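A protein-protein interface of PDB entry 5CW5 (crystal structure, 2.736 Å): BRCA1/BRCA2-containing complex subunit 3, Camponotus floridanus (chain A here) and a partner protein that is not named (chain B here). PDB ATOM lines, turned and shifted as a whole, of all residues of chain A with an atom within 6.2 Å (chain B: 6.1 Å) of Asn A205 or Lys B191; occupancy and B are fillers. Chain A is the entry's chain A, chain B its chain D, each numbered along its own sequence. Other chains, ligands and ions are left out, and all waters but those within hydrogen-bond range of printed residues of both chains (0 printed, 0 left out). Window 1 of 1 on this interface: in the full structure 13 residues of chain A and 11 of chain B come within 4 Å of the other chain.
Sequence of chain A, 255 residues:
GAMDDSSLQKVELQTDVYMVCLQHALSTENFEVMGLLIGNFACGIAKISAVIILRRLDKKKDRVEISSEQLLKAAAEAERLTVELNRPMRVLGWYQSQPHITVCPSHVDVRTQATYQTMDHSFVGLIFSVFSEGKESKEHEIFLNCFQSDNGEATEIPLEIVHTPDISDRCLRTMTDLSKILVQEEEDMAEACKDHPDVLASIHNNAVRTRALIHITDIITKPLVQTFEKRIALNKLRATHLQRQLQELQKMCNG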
ATOM      1  N   ALA A 190      11.368 -12.586  15.947  1.00  0.00           N
ATOM      2  CA  ALA A 190      11.653 -14.000  16.156  1.00  0.00           C
ATOM      3  C   ALA A 190      10.431 -14.859  15.849  1.00  0.00           C
ATOM      4  O   ALA A 190      10.552 -16.054  15.586  1.00  0.00           O
ATOM      5  CB  ALA A 190      12.122 -14.238  17.578  1.00  0.00           C
ATOM      6  N   CYS A 193      10.349 -16.014  12.230  1.00  0.00           N
ATOM      7  CA  CYS A 193      11.366 -17.016  11.936  1.00  0.00           C
ATOM      8  C   CYS A 193      11.179 -18.263  12.793  1.00  0.00           C
ATOM      9  O   CYS A 193      12.010 -19.171  12.773  1.00  0.00           O
ATOM     10  CB  CYS A 193      12.766 -16.436  12.151  1.00  0.00           C
ATOM     11  SG  CYS A 193      13.119 -14.973  11.151  1.00  0.00           S
ATOM     12  N   LYS A 194      10.083 -18.298  13.543  1.00  0.00           N
ATOM     13  CA  LYS A 194       9.781 -19.430  14.409  1.00  0.00           C
ATOM     14  C   LYS A 194       9.459 -20.679  13.594  1.00  0.00           C
ATOM     15  O   LYS A 194       9.123 -20.589  12.412  1.00  0.00           O
ATOM     16  CB  LYS A 194       8.614 -19.096  15.341  1.00  0.00           C
ATOM     17  N   HIS A 196      11.411 -23.088  12.433  1.00  0.00           N
ATOM     18  CA  HIS A 196      12.315 -23.307  11.311  1.00  0.00           C
ATOM     19  C   HIS A 196      12.701 -24.779  11.250  1.00  0.00           C
ATOM     20  O   HIS A 196      13.136 -25.350  12.255  1.00  0.00           O
ATOM     21  CB  HIS A 196      13.561 -22.429  11.441  1.00  0.00           C
ATOM     22  CG  HIS A 196      14.334 -22.276  10.167  1.00  0.00           C
ATOM     23  ND1 HIS A 196      14.958 -23.334   9.542  1.00  0.00           N
ATOM     24  CD2 HIS A 196      14.593 -21.186   9.408  1.00  0.00           C
ATOM     25  CE1 HIS A 196      15.561 -22.904   8.449  1.00  0.00           C
ATOM     26  NE2 HIS A 196      15.358 -21.603   8.345  1.00  0.00           N
ATOM     27  N   LEU A 200      20.014 -26.308  12.872  1.00  0.00           N
ATOM     28  CA  LEU A 200      21.085 -25.329  13.024  1.00  0.00           C
ATOM     29  C   LEU A 200      20.549 -23.900  12.977  1.00  0.00           C
ATOM     30  O   LEU A 200      21.091 -23.004  13.624  1.00  0.00           O
ATOM     31  CB  LEU A 200      22.151 -25.526  11.943  1.00  0.00           C
ATOM     32  CG  LEU A 200      22.837 -26.893  11.895  1.00  0.00           C
ATOM     33  CD1 LEU A 200      23.879 -26.934  10.787  1.00  0.00           C
ATOM     34  CD2 LEU A 200      23.466 -27.223  13.238  1.00  0.00           C
ATOM     35  N   ALA A 201      19.479 -23.694  12.217  1.00  0.00           N
ATOM     36  CA  ALA A 201      18.861 -22.376  12.106  1.00  0.00           C
ATOM     37  C   ALA A 201      18.055 -22.041  13.357  1.00  0.00           C
ATOM     38  O   ALA A 201      18.035 -20.894  13.803  1.00  0.00           O
ATOM     39  CB  ALA A 201      17.978 -22.306  10.872  1.00  0.00           C
ATOM     40  N   SER A 202      17.389 -23.049  13.915  1.00  0.00           N
ATOM     41  CA  SER A 202      16.612 -22.869  15.137  1.00  0.00           C
ATOM     42  C   SER A 202      17.523 -22.511  16.304  1.00  0.00           C
ATOM     43  O   SER A 202      17.192 -21.653  17.120  1.00  0.00           O
ATOM     44  CB  SER A 202      15.812 -24.131  15.461  1.00  0.00           C
ATOM     45  OG  SER A 202      14.917 -24.455  14.411  1.00  0.00           O
ATOM     46  N   ILE A 203      18.672 -23.177  16.373  1.00  0.00           N
ATOM     47  CA  ILE A 203      19.662 -22.897  17.405  1.00  0.00           C
ATOM     48  C   ILE A 203      20.219 -21.487  17.225  1.00  0.00           C
ATOM     49  O   ILE A 203      20.406 -20.753  18.197  1.00  0.00           O
ATOM     50  CB  ILE A 203      20.812 -23.924  17.377  1.00  0.00           C
ATOM     51  CG1 ILE A 203      20.269 -25.335  17.604  1.00  0.00           C
ATOM     52  CG2 ILE A 203      21.854 -23.592  18.428  1.00  0.00           C
ATOM     53  CD1 ILE A 203      21.328 -26.413  17.544  1.00  0.00           C
ATOM     54  N   HIS A 204      20.465 -21.112  15.974  1.00  0.00           N
ATOM     55  CA  HIS A 204      20.956 -19.775  15.649  1.00  0.00           C
ATOM     56  C   HIS A 204      19.950 -18.695  16.041  1.00  0.00           C
ATOM     57  O   HIS A 204      20.319 -17.689  16.646  1.00  0.00           O
ATOM     58  CB  HIS A 204      21.274 -19.675  14.155  1.00  0.00           C
ATOM     59  CG  HIS A 204      21.779 -18.329  13.732  1.00  0.00           C
ATOM     60  ND1 HIS A 204      23.115 -17.991  13.766  1.00  0.00           N
ATOM     61  CD2 HIS A 204      21.128 -17.238  13.265  1.00  0.00           C
ATOM     62  CE1 HIS A 204      23.264 -16.751  13.337  1.00  0.00           C
ATOM     63  NE2 HIS A 204      22.073 -16.271  13.028  1.00  0.00           N
ATOM     64  N   ASN A 205      18.684 -18.909  15.692  1.00  0.00           N
ATOM     65  CA  ASN A 205      17.629 -17.944  15.994  1.00  0.00           C
ATOM     66  C   ASN A 205      17.395 -17.775  17.492  1.00  0.00           C
ATOM     67  O   ASN A 205      17.176 -16.662  17.969  1.00  0.00           O
ATOM     68  CB  ASN A 205      16.322 -18.354  15.314  1.00  0.00           C
ATOM     69  CG  ASN A 205      16.351 -18.136  13.816  1.00  0.00           C
ATOM     70  OD1 ASN A 205      17.117 -17.316  13.310  1.00  0.00           O
ATOM     71  ND2 ASN A 205      15.507 -18.868  13.096  1.00  0.00           N
ATOM     72  N   ASN A 206      17.434 -18.880  18.229  1.00  0.00           N
ATOM     73  CA  ASN A 206      17.279 -18.831  19.678  1.00  0.00           C
ATOM     74  C   ASN A 206      18.485 -18.182  20.344  1.00  0.00           C
ATOM     75  O   ASN A 206      18.379 -17.620  21.432  1.00  0.00           O
ATOM     76  CB  ASN A 206      17.057 -20.234  20.245  1.00  0.00           C
ATOM     77  CG  ASN A 206      15.728 -20.827  19.826  1.00  0.00           C
ATOM     78  OD1 ASN A 206      14.771 -20.102  19.549  1.00  0.00           O
ATOM     79  ND2 ASN A 206      15.660 -22.152  19.780  1.00  0.00           N
ATOM     80  N   ALA A 207      19.634 -18.268  19.682  1.00  0.00           N
ATOM     81  CA  ALA A 207      20.844 -17.622  20.172  1.00  0.00           C
ATOM     82  C   ALA A 207      20.757 -16.118  19.951  1.00  0.00           C
ATOM     83  O   ALA A 207      21.172 -15.329  20.800  1.00  0.00           O
ATOM     84  CB  ALA A 207      22.073 -18.195  19.483  1.00  0.00           C
ATOM     85  N   VAL A 208      20.211 -15.731  18.802  1.00  0.00           N
ATOM     86  CA  VAL A 208      20.032 -14.325  18.464  1.00  0.00           C
ATOM     87  C   VAL A 208      19.004 -13.671  19.382  1.00  0.00           C
ATOM     88  O   VAL A 208      19.219 -12.566  19.883  1.00  0.00           O
ATOM     89  CB  VAL A 208      19.598 -14.153  16.992  1.00  0.00           C
ATOM     90  CG1 VAL A 208      19.123 -12.730  16.730  1.00  0.00           C
ATOM     91  CG2 VAL A 208      20.739 -14.524  16.057  1.00  0.00           C
ATOM     92  N   ARG A 209      17.894 -14.365  19.609  1.00  0.00           N
ATOM     93  CA  ARG A 209      16.835 -13.854  20.469  1.00  0.00           C
ATOM     94  C   ARG A 209      17.319 -13.702  21.907  1.00  0.00           C
ATOM     95  O   ARG A 209      16.990 -12.726  22.581  1.00  0.00           O
ATOM     96  CB  ARG A 209      15.612 -14.772  20.422  1.00  0.00           C
ATOM     97  CG  ARG A 209      14.350 -14.154  21.003  1.00  0.00           C
ATOM     98  CD  ARG A 209      13.165 -15.095  20.867  1.00  0.00           C
ATOM     99  NE  ARG A 209      13.027 -15.990  22.011  1.00  0.00           N
ATOM    100  CZ  ARG A 209      11.956 -16.032  22.797  1.00  0.00           C
ATOM    101  NH1 ARG A 209      10.926 -15.235  22.553  1.00  0.00           N
ATOM    102  NH2 ARG A 209      11.910 -16.874  23.819  1.00  0.00           N
ATOM    103  N   THR A 210      18.108 -14.668  22.368  1.00  0.00           N
ATOM    104  CA  THR A 210      18.631 -14.651  23.730  1.00  0.00           C
ATOM    105  C   THR A 210      19.536 -13.447  23.970  1.00  0.00           C
ATOM    106  O   THR A 210      19.364 -12.717  24.946  1.00  0.00           O
ATOM    107  CB  THR A 210      19.416 -15.935  24.049  1.00  0.00           C
ATOM    108  OG1 THR A 210      18.567 -17.076  23.871  1.00  0.00           O
ATOM    109  CG2 THR A 210      19.921 -15.908  25.482  1.00  0.00           C
ATOM    110  N   ASP B 181      27.530 -14.380   4.264  1.00  0.00           N
ATOM    111  CA  ASP B 181      26.770 -15.392   3.538  1.00  0.00           C
ATOM    112  C   ASP B 181      25.458 -14.801   3.025  1.00  0.00           C
ATOM    113  O   ASP B 181      25.164 -13.630   3.261  1.00  0.00           O
ATOM    114  CB  ASP B 181      26.505 -16.613   4.422  1.00  0.00           C
ATOM    115  CG  ASP B 181      25.896 -16.246   5.759  1.00  0.00           C
ATOM    116  OD1 ASP B 181      26.661 -15.932   6.695  1.00  0.00           O
ATOM    117  OD2 ASP B 181      24.653 -16.279   5.876  1.00  0.00           O
ATOM    118  N   SER B 183      22.449 -15.295   3.860  1.00  0.00           N
ATOM    119  CA  SER B 183      21.368 -15.153   4.829  1.00  0.00           C
ATOM    120  C   SER B 183      21.530 -13.875   5.646  1.00  0.00           C
ATOM    121  O   SER B 183      21.158 -13.823   6.818  1.00  0.00           O
ATOM    122  CB  SER B 183      21.309 -16.366   5.757  1.00  0.00           C
ATOM    123  OG  SER B 183      22.472 -16.450   6.561  1.00  0.00           O
ATOM    124  N   SER B 188      18.387  -8.050   9.422  1.00  0.00           N
ATOM    125  CA  SER B 188      18.406  -8.667  10.743  1.00  0.00           C
ATOM    126  C   SER B 188      19.368  -9.848  10.782  1.00  0.00           C
ATOM    127  O   SER B 188      19.848 -10.305   9.745  1.00  0.00           O
ATOM    128  CB  SER B 188      17.002  -9.121  11.144  1.00  0.00           C
ATOM    129  OG  SER B 188      16.521 -10.117  10.258  1.00  0.00           O
ATOM    130  N   ASP B 189      19.643 -10.338  11.986  1.00  0.00           N
ATOM    131  CA  ASP B 189      20.550 -11.465  12.166  1.00  0.00           C
ATOM    132  C   ASP B 189      19.797 -12.790  12.188  1.00  0.00           C
ATOM    133  O   ASP B 189      20.404 -13.856  12.275  1.00  0.00           O
ATOM    134  CB  ASP B 189      21.364 -11.297  13.453  1.00  0.00           C
ATOM    135  CG  ASP B 189      22.234 -10.055  13.436  1.00  0.00           C
ATOM    136  OD1 ASP B 189      22.586  -9.595  12.332  1.00  0.00           O
ATOM    137  OD2 ASP B 189      22.566  -9.543  14.525  1.00  0.00           O
ATOM    138  N   TYR B 190      18.472 -12.718  12.116  1.00  0.00           N
ATOM    139  CA  TYR B 190      17.651 -13.920  12.089  1.00  0.00           C
ATOM    140  C   TYR B 190      17.726 -14.604  10.731  1.00  0.00           C
ATOM    141  O   TYR B 190      18.036 -13.973   9.722  1.00  0.00           O
ATOM    142  CB  TYR B 190      16.195 -13.596  12.418  1.00  0.00           C
ATOM    143  CG  TYR B 190      15.943 -13.249  13.865  1.00  0.00           C
ATOM    144  CD1 TYR B 190      15.910 -14.237  14.838  1.00  0.00           C
ATOM    145  CD2 TYR B 190      15.718 -11.936  14.253  1.00  0.00           C
ATOM    146  CE1 TYR B 190      15.673 -13.927  16.161  1.00  0.00           C
ATOM    147  CE2 TYR B 190      15.479 -11.615  15.572  1.00  0.00           C
ATOM    148  CZ  TYR B 190      15.457 -12.613  16.522  1.00  0.00           C
ATOM    149  OH  TYR B 190      15.221 -12.296  17.838  1.00  0.00           O
ATOM    150  N   LYS B 191      17.439 -15.902  10.716  1.00  0.00           N
ATOM    151  CA  LYS B 191      17.375 -16.669   9.478  1.00  0.00           C
ATOM    152  C   LYS B 191      15.924 -16.985   9.145  1.00  0.00           C
ATOM    153  O   LYS B 191      15.310 -17.844   9.778  1.00  0.00           O
ATOM    154  CB  LYS B 191      18.192 -17.959   9.588  1.00  0.00           C
ATOM    155  CG  LYS B 191      19.695 -17.742   9.662  1.00  0.00           C
ATOM    156  CD  LYS B 191      20.438 -19.058   9.857  1.00  0.00           C
ATOM    157  CE  LYS B 191      21.947 -18.852   9.806  1.00  0.00           C
ATOM    158  NZ  LYS B 191      22.402 -18.362   8.475  1.00  0.00           N
ATOM    159  N   PRO B 192      15.371 -16.284   8.146  1.00  0.00           N
ATOM    160  CA  PRO B 192      13.960 -16.420   7.774  1.00  0.00           C
ATOM    161  C   PRO B 192      13.634 -17.794   7.204  1.00  0.00           C
ATOM    162  O   PRO B 192      14.435 -18.361   6.462  1.00  0.00           O
ATOM    163  CB  PRO B 192      13.772 -15.331   6.714  1.00  0.00           C
ATOM    164  CG  PRO B 192      15.132 -15.137   6.137  1.00  0.00           C
ATOM    165  CD  PRO B 192      16.079 -15.323   7.285  1.00  0.00           C
ATOM    166  N   THR B 193      12.469 -18.321   7.561  1.00  0.00           N
ATOM    167  CA  THR B 193      12.021 -19.607   7.046  1.00  0.00           C
ATOM    168  C   THR B 193      11.605 -19.481   5.582  1.00  0.00           C
ATOM    169  O   THR B 193      10.757 -18.655   5.245  1.00  0.00           O
ATOM    170  CB  THR B 193      10.842 -20.160   7.866  1.00  0.00           C
ATOM    171  OG1 THR B 193       9.726 -19.269   7.761  1.00  0.00           O
ATOM    172  CG2 THR B 193      11.231 -20.300   9.329  1.00  0.00           C
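Of the printed residues of chain B, His A196 touches Lys B191, Pro B192 and Thr B193.
Asn A205 touches two residues of chain B.
Of the printed residues of chain B, Arg A209 touches Tyr B190 (3.5 Å).
Thr A210 touches none of the printed residues of chain B.
Printed residues of chain A within 4 Å of Tyr B190: Ala A190, Cys A193, Asn A205, Val A208 and Arg A209.
Lys B191 touches just these residues of chain A: Cys A193, His A196, His A204 and Asn A205.
Of the printed residues of chain A, Pro B192 touches Cys A193 (3.8 Å) and His A196 (3.9 Å).
Of the printed residues of chain A, Thr B193 touches Cys A193, Lys A194 and His A196.
The nearest printed residue of chain B that does not touch Cys A193 is Ser B188 (6.0 Å).
The side-chain hydroxyl (OG) of Ser B183 is in hydrogen-bond range of the side-chain amino group (NZ) of Lys B191 (2.7 Å).
The backbone carbonyl oxygen (O) of Ala A201 sits close to the side-chain amide nitrogen (ND2) of Asn A205 (3.3 Å).
The backbone carbonyl oxygen (O) of His A196 is in hydrogen-bond range of the side-chain hydroxyl (OG) of Ser A202, 2.9 Å away.
A ring nitrogen (NE2) of His A204 sits at hydrogen-bond distance from the backbone carbonyl oxygen of Asp B189 (3.0 Å).
The side-chain amide oxygen (OD1) of Asn A205 sits at hydrogen-bond distance from the backbone NH (N) of Lys B191 (3.0 Å).
SG of Cys A193 touches CB of Tyr B190, 3.6 Å away.
SG of Cys A193 touches CA of Pro B192, 3.8 Å away.
Thr B193 touches Cys A193 (CG2 to O, 3.7 Å).
O of Lys A194 touches CG2 of Thr B193, 3.7 Å away.
O of Pro B192 touches NE2 of His A196, at 3.9 Å.
His A196 touches Thr B193.
Lys B191 touches His A204.
O of Asp B189 touches CG2 of Val A208, 3.9 Å away.
Tyr B190 touches Val A208.
Tyr B190 touches Arg A209 (OH to CA, 3.5 Å).
Of the 8 printed residues of chain B, 5 touch a printed residue of chain A.
Hydrophobic or aromatic side chains of chain B that line the printed part of chain A: Tyr B190.
Of the 15 printed residues of chain A, 8 touch a printed residue of chain B.
Hydrophobic or aromatic side chains of chain A that line the printed part of chain B: Ala A190, His A196, His A204 and Val A208.
Among the printed residues, no Asp or Glu carboxylate lies within 4 Å of a Lys or Arg side-chain nitrogen of the other chain.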
